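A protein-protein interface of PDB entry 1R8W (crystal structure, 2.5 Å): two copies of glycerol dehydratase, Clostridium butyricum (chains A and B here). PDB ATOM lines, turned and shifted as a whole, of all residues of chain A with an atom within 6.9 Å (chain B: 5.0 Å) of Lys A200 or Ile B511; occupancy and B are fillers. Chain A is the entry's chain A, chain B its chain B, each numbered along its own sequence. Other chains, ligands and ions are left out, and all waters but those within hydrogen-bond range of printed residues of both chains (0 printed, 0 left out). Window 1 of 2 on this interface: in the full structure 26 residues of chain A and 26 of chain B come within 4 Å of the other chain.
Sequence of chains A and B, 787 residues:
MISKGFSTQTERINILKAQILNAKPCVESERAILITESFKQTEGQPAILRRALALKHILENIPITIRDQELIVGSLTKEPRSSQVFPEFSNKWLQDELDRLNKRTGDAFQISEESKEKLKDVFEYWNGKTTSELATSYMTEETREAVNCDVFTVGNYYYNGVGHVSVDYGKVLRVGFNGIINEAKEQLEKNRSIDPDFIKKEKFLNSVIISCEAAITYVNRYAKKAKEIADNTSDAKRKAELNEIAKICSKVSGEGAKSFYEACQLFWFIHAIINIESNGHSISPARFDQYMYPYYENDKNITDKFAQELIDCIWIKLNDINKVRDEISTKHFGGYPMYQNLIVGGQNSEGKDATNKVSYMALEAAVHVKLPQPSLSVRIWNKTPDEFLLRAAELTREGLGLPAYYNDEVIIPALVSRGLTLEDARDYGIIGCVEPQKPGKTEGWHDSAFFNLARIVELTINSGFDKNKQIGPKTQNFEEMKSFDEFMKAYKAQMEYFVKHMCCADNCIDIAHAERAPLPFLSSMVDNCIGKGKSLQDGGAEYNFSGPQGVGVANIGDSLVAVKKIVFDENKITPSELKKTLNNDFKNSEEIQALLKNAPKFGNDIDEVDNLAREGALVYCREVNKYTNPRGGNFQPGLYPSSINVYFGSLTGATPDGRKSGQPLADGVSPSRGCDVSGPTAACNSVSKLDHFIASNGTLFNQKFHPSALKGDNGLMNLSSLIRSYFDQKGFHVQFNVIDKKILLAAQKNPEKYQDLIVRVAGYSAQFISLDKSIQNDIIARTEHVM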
ATOM      1  N   ILE A  48      25.472   8.719 -18.164  1.00  0.00           N
ATOM      2  CA  ILE A  48      25.784   7.403 -17.615  1.00  0.00           C
ATOM      3  C   ILE A  48      27.281   7.217 -17.364  1.00  0.00           C
ATOM      4  O   ILE A  48      27.678   6.550 -16.406  1.00  0.00           O
ATOM      5  CB  ILE A  48      25.261   6.262 -18.542  1.00  0.00           C
ATOM      6  CG1 ILE A  48      25.323   4.923 -17.805  1.00  0.00           C
ATOM      7  CG2 ILE A  48      26.085   6.188 -19.819  1.00  0.00           C
ATOM      8  CD1 ILE A  48      24.395   4.835 -16.614  1.00  0.00           C
ATOM      9  N   PRO A 196      22.134   1.970 -34.786  1.00  0.00           N
ATOM     10  CA  PRO A 196      22.411   3.151 -33.956  1.00  0.00           C
ATOM     11  C   PRO A 196      22.101   2.935 -32.473  1.00  0.00           C
ATOM     12  O   PRO A 196      22.776   3.488 -31.606  1.00  0.00           O
ATOM     13  CB  PRO A 196      21.515   4.229 -34.564  1.00  0.00           C
ATOM     14  CG  PRO A 196      21.359   3.800 -35.975  1.00  0.00           C
ATOM     15  CD  PRO A 196      21.189   2.306 -35.865  1.00  0.00           C
ATOM     16  N   ASP A 197      21.074   2.135 -32.190  1.00  0.00           N
ATOM     17  CA  ASP A 197      20.674   1.850 -30.817  1.00  0.00           C
ATOM     18  C   ASP A 197      21.791   1.285 -29.967  1.00  0.00           C
ATOM     19  O   ASP A 197      21.801   1.462 -28.753  1.00  0.00           O
ATOM     20  CB  ASP A 197      19.498   0.875 -30.787  1.00  0.00           C
ATOM     21  CG  ASP A 197      18.169   1.564 -31.025  1.00  0.00           C
ATOM     22  OD1 ASP A 197      17.914   2.598 -30.363  1.00  0.00           O
ATOM     23  OD2 ASP A 197      17.380   1.071 -31.866  1.00  0.00           O
ATOM     24  N   PHE A 198      22.734   0.601 -30.596  1.00  0.00           N
ATOM     25  CA  PHE A 198      23.830   0.012 -29.849  1.00  0.00           C
ATOM     26  C   PHE A 198      24.755   1.060 -29.228  1.00  0.00           C
ATOM     27  O   PHE A 198      25.392   0.798 -28.207  1.00  0.00           O
ATOM     28  CB  PHE A 198      24.629  -0.941 -30.749  1.00  0.00           C
ATOM     29  CG  PHE A 198      25.845  -1.528 -30.083  1.00  0.00           C
ATOM     30  CD1 PHE A 198      27.124  -1.073 -30.412  1.00  0.00           C
ATOM     31  CD2 PHE A 198      25.712  -2.517 -29.106  1.00  0.00           C
ATOM     32  CE1 PHE A 198      28.255  -1.591 -29.777  1.00  0.00           C
ATOM     33  CE2 PHE A 198      26.835  -3.041 -28.465  1.00  0.00           C
ATOM     34  CZ  PHE A 198      28.109  -2.577 -28.800  1.00  0.00           C
ATOM     35  N   ILE A 199      24.818   2.246 -29.830  1.00  0.00           N
ATOM     36  CA  ILE A 199      25.686   3.305 -29.320  1.00  0.00           C
ATOM     37  C   ILE A 199      25.445   3.612 -27.844  1.00  0.00           C
ATOM     38  O   ILE A 199      26.383   3.612 -27.049  1.00  0.00           O
ATOM     39  CB  ILE A 199      25.533   4.604 -30.148  1.00  0.00           C
ATOM     40  CG1 ILE A 199      25.977   4.338 -31.592  1.00  0.00           C
ATOM     41  CG2 ILE A 199      26.364   5.731 -29.522  1.00  0.00           C
ATOM     42  CD1 ILE A 199      25.707   5.473 -32.555  1.00  0.00           C
ATOM     43  N   LYS A 200      24.195   3.866 -27.474  1.00  0.00           N
ATOM     44  CA  LYS A 200      23.877   4.159 -26.084  1.00  0.00           C
ATOM     45  C   LYS A 200      23.982   2.921 -25.198  1.00  0.00           C
ATOM     46  O   LYS A 200      24.332   3.031 -24.027  1.00  0.00           O
ATOM     47  CB  LYS A 200      22.475   4.762 -25.961  1.00  0.00           C
ATOM     48  CG  LYS A 200      22.349   6.144 -26.572  1.00  0.00           C
ATOM     49  CD  LYS A 200      21.074   6.829 -26.126  1.00  0.00           C
ATOM     50  CE  LYS A 200      20.990   8.246 -26.679  1.00  0.00           C
ATOM     51  NZ  LYS A 200      19.861   9.025 -26.078  1.00  0.00           N
ATOM     52  N   LYS A 201      23.680   1.747 -25.744  1.00  0.00           N
ATOM     53  CA  LYS A 201      23.766   0.524 -24.953  1.00  0.00           C
ATOM     54  C   LYS A 201      25.217   0.257 -24.589  1.00  0.00           C
ATOM     55  O   LYS A 201      25.516  -0.172 -23.474  1.00  0.00           O
ATOM     56  CB  LYS A 201      23.222  -0.676 -25.723  1.00  0.00           C
ATOM     57  CG  LYS A 201      21.751  -0.590 -26.087  1.00  0.00           C
ATOM     58  CD  LYS A 201      21.262  -1.932 -26.626  1.00  0.00           C
ATOM     59  CE  LYS A 201      19.883  -1.821 -27.257  1.00  0.00           C
ATOM     60  NZ  LYS A 201      18.862  -1.268 -26.321  1.00  0.00           N
ATOM     61  N   GLU A 202      26.123   0.516 -25.527  1.00  0.00           N
ATOM     62  CA  GLU A 202      27.535   0.285 -25.270  1.00  0.00           C
ATOM     63  C   GLU A 202      28.026   1.169 -24.133  1.00  0.00           C
ATOM     64  O   GLU A 202      28.750   0.709 -23.250  1.00  0.00           O
ATOM     65  CB  GLU A 202      28.385   0.555 -26.511  1.00  0.00           C
ATOM     66  CG  GLU A 202      29.845   0.221 -26.263  1.00  0.00           C
ATOM     67  CD  GLU A 202      30.783   0.850 -27.259  1.00  0.00           C
ATOM     68  OE1 GLU A 202      30.814   2.099 -27.342  1.00  0.00           O
ATOM     69  OE2 GLU A 202      31.495   0.093 -27.953  1.00  0.00           O
ATOM     70  N   LYS A 203      27.641   2.440 -24.163  1.00  0.00           N
ATOM     71  CA  LYS A 203      28.049   3.363 -23.118  1.00  0.00           C
ATOM     72  C   LYS A 203      27.558   2.867 -21.766  1.00  0.00           C
ATOM     73  O   LYS A 203      28.277   2.939 -20.770  1.00  0.00           O
ATOM     74  CB  LYS A 203      27.511   4.765 -23.410  1.00  0.00           C
ATOM     75  CG  LYS A 203      28.080   5.351 -24.695  1.00  0.00           C
ATOM     76  CD  LYS A 203      29.607   5.287 -24.687  1.00  0.00           C
ATOM     77  CE  LYS A 203      30.176   5.210 -26.095  1.00  0.00           C
ATOM     78  NZ  LYS A 203      31.669   5.163 -26.077  1.00  0.00           N
ATOM     79  N   PHE A 204      26.338   2.343 -21.735  1.00  0.00           N
ATOM     80  CA  PHE A 204      25.788   1.832 -20.495  1.00  0.00           C
ATOM     81  C   PHE A 204      26.599   0.637 -19.997  1.00  0.00           C
ATOM     82  O   PHE A 204      27.014   0.593 -18.837  1.00  0.00           O
ATOM     83  CB  PHE A 204      24.324   1.404 -20.681  1.00  0.00           C
ATOM     84  CG  PHE A 204      23.755   0.699 -19.481  1.00  0.00           C
ATOM     85  CD1 PHE A 204      23.500   1.398 -18.304  1.00  0.00           C
ATOM     86  CD2 PHE A 204      23.555  -0.679 -19.499  1.00  0.00           C
ATOM     87  CE1 PHE A 204      23.060   0.732 -17.156  1.00  0.00           C
ATOM     88  CE2 PHE A 204      23.115  -1.355 -18.357  1.00  0.00           C
ATOM     89  CZ  PHE A 204      22.870  -0.644 -17.182  1.00  0.00           C
ATOM     90  N   LEU A 205      26.817  -0.337 -20.874  1.00  0.00           N
ATOM     91  CA  LEU A 205      27.565  -1.527 -20.496  1.00  0.00           C
ATOM     92  C   LEU A 205      28.987  -1.199 -20.046  1.00  0.00           C
ATOM     93  O   LEU A 205      29.480  -1.787 -19.089  1.00  0.00           O
ATOM     94  CB  LEU A 205      27.570  -2.528 -21.651  1.00  0.00           C
ATOM     95  CG  LEU A 205      26.179  -3.092 -21.965  1.00  0.00           C
ATOM     96  CD1 LEU A 205      26.207  -3.902 -23.247  1.00  0.00           C
ATOM     97  CD2 LEU A 205      25.704  -3.940 -20.798  1.00  0.00           C
ATOM     98  N   GLY A 533      20.560  -3.415 -21.863  1.00  0.00           N
ATOM     99  CA  GLY A 533      21.497  -2.321 -22.060  1.00  0.00           C
ATOM    100  C   GLY A 533      20.895  -0.996 -21.630  1.00  0.00           C
ATOM    101  O   GLY A 533      21.216   0.053 -22.185  1.00  0.00           O
ATOM    102  N   LYS A 534      20.017  -1.052 -20.634  1.00  0.00           N
ATOM    103  CA  LYS A 534      19.339   0.131 -20.115  1.00  0.00           C
ATOM    104  C   LYS A 534      19.453   0.178 -18.602  1.00  0.00           C
ATOM    105  O   LYS A 534      19.401  -0.858 -17.945  1.00  0.00           O
ATOM    106  CB  LYS A 534      17.847   0.090 -20.443  1.00  0.00           C
ATOM    107  CG  LYS A 534      17.438   0.351 -21.867  1.00  0.00           C
ATOM    108  CD  LYS A 534      15.919   0.351 -21.909  1.00  0.00           C
ATOM    109  CE  LYS A 534      15.358   0.702 -23.274  1.00  0.00           C
ATOM    110  NZ  LYS A 534      13.858   0.645 -23.238  1.00  0.00           N
ATOM    111  N   TYR B 138      30.815   9.692 -27.463  1.00  0.00           N
ATOM    112  CA  TYR B 138      29.943   8.596 -27.876  1.00  0.00           C
ATOM    113  C   TYR B 138      30.639   7.583 -28.783  1.00  0.00           C
ATOM    114  O   TYR B 138      30.255   6.419 -28.829  1.00  0.00           O
ATOM    115  CB  TYR B 138      28.704   9.141 -28.587  1.00  0.00           C
ATOM    116  CG  TYR B 138      27.544   9.404 -27.657  1.00  0.00           C
ATOM    117  CD1 TYR B 138      27.011  10.685 -27.516  1.00  0.00           C
ATOM    118  CD2 TYR B 138      26.980   8.369 -26.906  1.00  0.00           C
ATOM    119  CE1 TYR B 138      25.943  10.929 -26.649  1.00  0.00           C
ATOM    120  CE2 TYR B 138      25.914   8.604 -26.039  1.00  0.00           C
ATOM    121  CZ  TYR B 138      25.401   9.886 -25.914  1.00  0.00           C
ATOM    122  OH  TYR B 138      24.357  10.124 -25.049  1.00  0.00           O
ATOM    123  N   ASN B 507      26.635   8.811 -36.933  1.00  0.00           N
ATOM    124  CA  ASN B 507      25.548   8.546 -35.995  1.00  0.00           C
ATOM    125  C   ASN B 507      25.844   9.050 -34.583  1.00  0.00           C
ATOM    126  O   ASN B 507      24.930   9.421 -33.852  1.00  0.00           O
ATOM    127  CB  ASN B 507      25.201   7.053 -35.967  1.00  0.00           C
ATOM    128  CG  ASN B 507      24.506   6.594 -37.242  1.00  0.00           C
ATOM    129  OD1 ASN B 507      23.903   7.399 -37.957  1.00  0.00           O
ATOM    130  ND2 ASN B 507      24.571   5.294 -37.523  1.00  0.00           N
ATOM    131  N   CYS B 508      27.113   9.073 -34.195  1.00  0.00           N
ATOM    132  CA  CYS B 508      27.455   9.570 -32.869  1.00  0.00           C
ATOM    133  C   CYS B 508      27.240  11.079 -32.870  1.00  0.00           C
ATOM    134  O   CYS B 508      26.778  11.656 -31.885  1.00  0.00           O
ATOM    135  CB  CYS B 508      28.909   9.237 -32.519  1.00  0.00           C
ATOM    136  SG  CYS B 508      29.200   7.478 -32.151  1.00  0.00           S
ATOM    137  N   ILE B 509      27.559  11.716 -33.992  1.00  0.00           N
ATOM    138  CA  ILE B 509      27.392  13.158 -34.130  1.00  0.00           C
ATOM    139  C   ILE B 509      25.904  13.481 -34.153  1.00  0.00           C
ATOM    140  O   ILE B 509      25.481  14.504 -33.623  1.00  0.00           O
ATOM    141  CB  ILE B 509      28.054  13.673 -35.433  1.00  0.00           C
ATOM    142  CG1 ILE B 509      29.554  13.371 -35.403  1.00  0.00           C
ATOM    143  CG2 ILE B 509      27.829  15.168 -35.587  1.00  0.00           C
ATOM    144  CD1 ILE B 509      30.258  13.662 -36.709  1.00  0.00           C
ATOM    145  N   ASP B 510      25.122  12.599 -34.773  1.00  0.00           N
ATOM    146  CA  ASP B 510      23.670  12.757 -34.875  1.00  0.00           C
ATOM    147  C   ASP B 510      23.084  12.810 -33.451  1.00  0.00           C
ATOM    148  O   ASP B 510      22.307  13.707 -33.114  1.00  0.00           O
ATOM    149  CB  ASP B 510      23.078  11.566 -35.649  1.00  0.00           C
ATOM    150  CG  ASP B 510      21.909  11.955 -36.550  1.00  0.00           C
ATOM    151  OD1 ASP B 510      21.013  12.700 -36.093  1.00  0.00           O
ATOM    152  OD2 ASP B 510      21.876  11.503 -37.717  1.00  0.00           O
ATOM    153  N   ILE B 511      23.482  11.846 -32.623  1.00  0.00           N
ATOM    154  CA  ILE B 511      23.031  11.751 -31.237  1.00  0.00           C
ATOM    155  C   ILE B 511      23.413  13.002 -30.448  1.00  0.00           C
ATOM    156  O   ILE B 511      22.618  13.523 -29.663  1.00  0.00           O
ATOM    157  CB  ILE B 511      23.685  10.546 -30.503  1.00  0.00           C
ATOM    158  CG1 ILE B 511      23.430   9.242 -31.263  1.00  0.00           C
ATOM    159  CG2 ILE B 511      23.163  10.459 -29.077  1.00  0.00           C
ATOM    160  CD1 ILE B 511      22.010   8.802 -31.275  1.00  0.00           C
ATOM    161  N   ALA B 512      24.639  13.472 -30.650  1.00  0.00           N
ATOM    162  CA  ALA B 512      25.135  14.642 -29.940  1.00  0.00           C
ATOM    163  C   ALA B 512      24.307  15.887 -30.213  1.00  0.00           C
ATOM    164  O   ALA B 512      24.033  16.672 -29.304  1.00  0.00           O
ATOM    165  CB  ALA B 512      26.587  14.891 -30.302  1.00  0.00           C
ATOM    166  N   HIS B 513      23.914  16.075 -31.468  1.00  0.00           N
ATOM    167  CA  HIS B 513      23.110  17.229 -31.836  1.00  0.00           C
ATOM    168  C   HIS B 513      21.721  17.147 -31.224  1.00  0.00           C
ATOM    169  O   HIS B 513      21.169  18.151 -30.773  1.00  0.00           O
ATOM    170  CB  HIS B 513      22.995  17.332 -33.354  1.00  0.00           C
ATOM    171  CG  HIS B 513      24.115  18.089 -33.987  1.00  0.00           C
ATOM    172  ND1 HIS B 513      24.234  19.457 -33.885  1.00  0.00           N
ATOM    173  CD2 HIS B 513      25.174  17.671 -34.720  1.00  0.00           C
ATOM    174  CE1 HIS B 513      25.318  19.851 -34.531  1.00  0.00           C
ATOM    175  NE2 HIS B 513      25.906  18.786 -35.046  1.00  0.00           N
ATOM    176  N   ALA B 514      21.154  15.951 -31.218  1.00  0.00           N
ATOM    177  CA  ALA B 514      19.832  15.765 -30.652  1.00  0.00           C
ATOM    178  C   ALA B 514      19.885  15.980 -29.144  1.00  0.00           C
ATOM    179  O   ALA B 514      18.936  16.472 -28.540  1.00  0.00           O
ATOM    180  CB  ALA B 514      19.330  14.361 -30.953  1.00  0.00           C
ATOM    181  N   GLU B 515      21.013  15.619 -28.545  1.00  0.00           N
ATOM    182  CA  GLU B 515      21.170  15.734 -27.107  1.00  0.00           C
ATOM    183  C   GLU B 515      21.517  17.129 -26.597  1.00  0.00           C
ATOM    184  O   GLU B 515      21.027  17.538 -25.547  1.00  0.00           O
ATOM    185  CB  GLU B 515      22.222  14.732 -26.634  1.00  0.00           C
ATOM    186  CG  GLU B 515      22.235  14.499 -25.142  1.00  0.00           C
ATOM    187  CD  GLU B 515      23.047  13.273 -24.757  1.00  0.00           C
ATOM    188  OE1 GLU B 515      22.891  12.224 -25.422  1.00  0.00           O
ATOM    189  OE2 GLU B 515      23.830  13.356 -23.784  1.00  0.00           O
ATOM    190  N   ARG B 516      22.346  17.866 -27.325  1.00  0.00           N
ATOM    191  CA  ARG B 516      22.727  19.192 -26.860  1.00  0.00           C
ATOM    192  C   ARG B 516      22.267  20.372 -27.700  1.00  0.00           C
ATOM    193  O   ARG B 516      22.316  21.506 -27.237  1.00  0.00           O
ATOM    194  CB  ARG B 516      24.244  19.261 -26.674  1.00  0.00           C
ATOM    195  CG  ARG B 516      24.735  18.363 -25.567  1.00  0.00           C
ATOM    196  CD  ARG B 516      26.214  18.535 -25.270  1.00  0.00           C
ATOM    197  NE  ARG B 516      26.563  17.785 -24.068  1.00  0.00           N
ATOM    198  CZ  ARG B 516      27.749  17.823 -23.473  1.00  0.00           C
ATOM    199  NH1 ARG B 516      28.715  18.578 -23.972  1.00  0.00           N
ATOM    200  NH2 ARG B 516      27.962  17.113 -22.374  1.00  0.00           N
ATOM    201  N   PRO B 630      20.129   7.527 -36.397  1.00  0.00           N
ATOM    202  CA  PRO B 630      19.323   7.557 -35.168  1.00  0.00           C
ATOM    203  C   PRO B 630      17.914   8.130 -35.331  1.00  0.00           C
ATOM    204  O   PRO B 630      17.063   7.967 -34.458  1.00  0.00           O
ATOM    205  CB  PRO B 630      20.176   8.401 -34.216  1.00  0.00           C
ATOM    206  CG  PRO B 630      21.569   8.191 -34.723  1.00  0.00           C
ATOM    207  CD  PRO B 630      21.379   8.283 -36.208  1.00  0.00           C
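The side-chain carboxylate (OE1) of Glu A202 lies within salt-bridge range of the side-chain amino group (NZ) of Lys A203, 3.4 Å away. The backbone carbonyl oxygen (O) of Tyr B138 is in hydrogen-bond range of the side-chain sulfur (SG) of Cys B508, 3.6 Å away. OH of Tyr B138 sits at hydrogen-bond distance from OE1 of Glu B515.
Among the printed residues, merely in contact across the chains: Pro A196 with Asn B507 (3.9 Å), Pro A196 with Pro B630 (3.9 Å), Ile A199 with Tyr B138 (3.8 Å), Ile A199 with Asn B507 (3.8 Å) and Lys A200 with Ile B511 (3.9 Å).
Hydrophobic or aromatic side chains of chain A that line the printed part of chain B: Pro A196 and Ile A199. Of the 12 printed residues of chain B, 4 touch a printed residue of chain A. Among the printed residues, 6 pairs touch across the chains.
NZ of Lys A203 lies close to O of Tyr B138.
Of the printed residues of chain B, Ile A199 touches Tyr B138 (3.8 Å) and Asn B507 (3.8 Å). Printed residues of chain B within 4 Å of Lys A200: Ile B511 (3.9 Å). Of the printed residues of chain B, Lys A203 touches Tyr B138. Of the printed residues of chain A, Tyr B138 touches Ile A199 and Lys A203. Of the printed residues of chain A, Asn B507 touches Pro A196 and Ile A199. Asp B510 touches none of the printed residues of chain A. Ile B511 touches one residue of chain A. His B513 touches none of the printed residues of chain A. Of the printed residues of chain A, Pro B630 touches Pro A196. The nearest residue of chain A that does not touch Ile B511 is Ile A199 (4.6 Å).
No position is printed for both chains. Of the 6 pairs that touch across the chains among the printed residues, none has its exchanged pair printed and touching as well.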
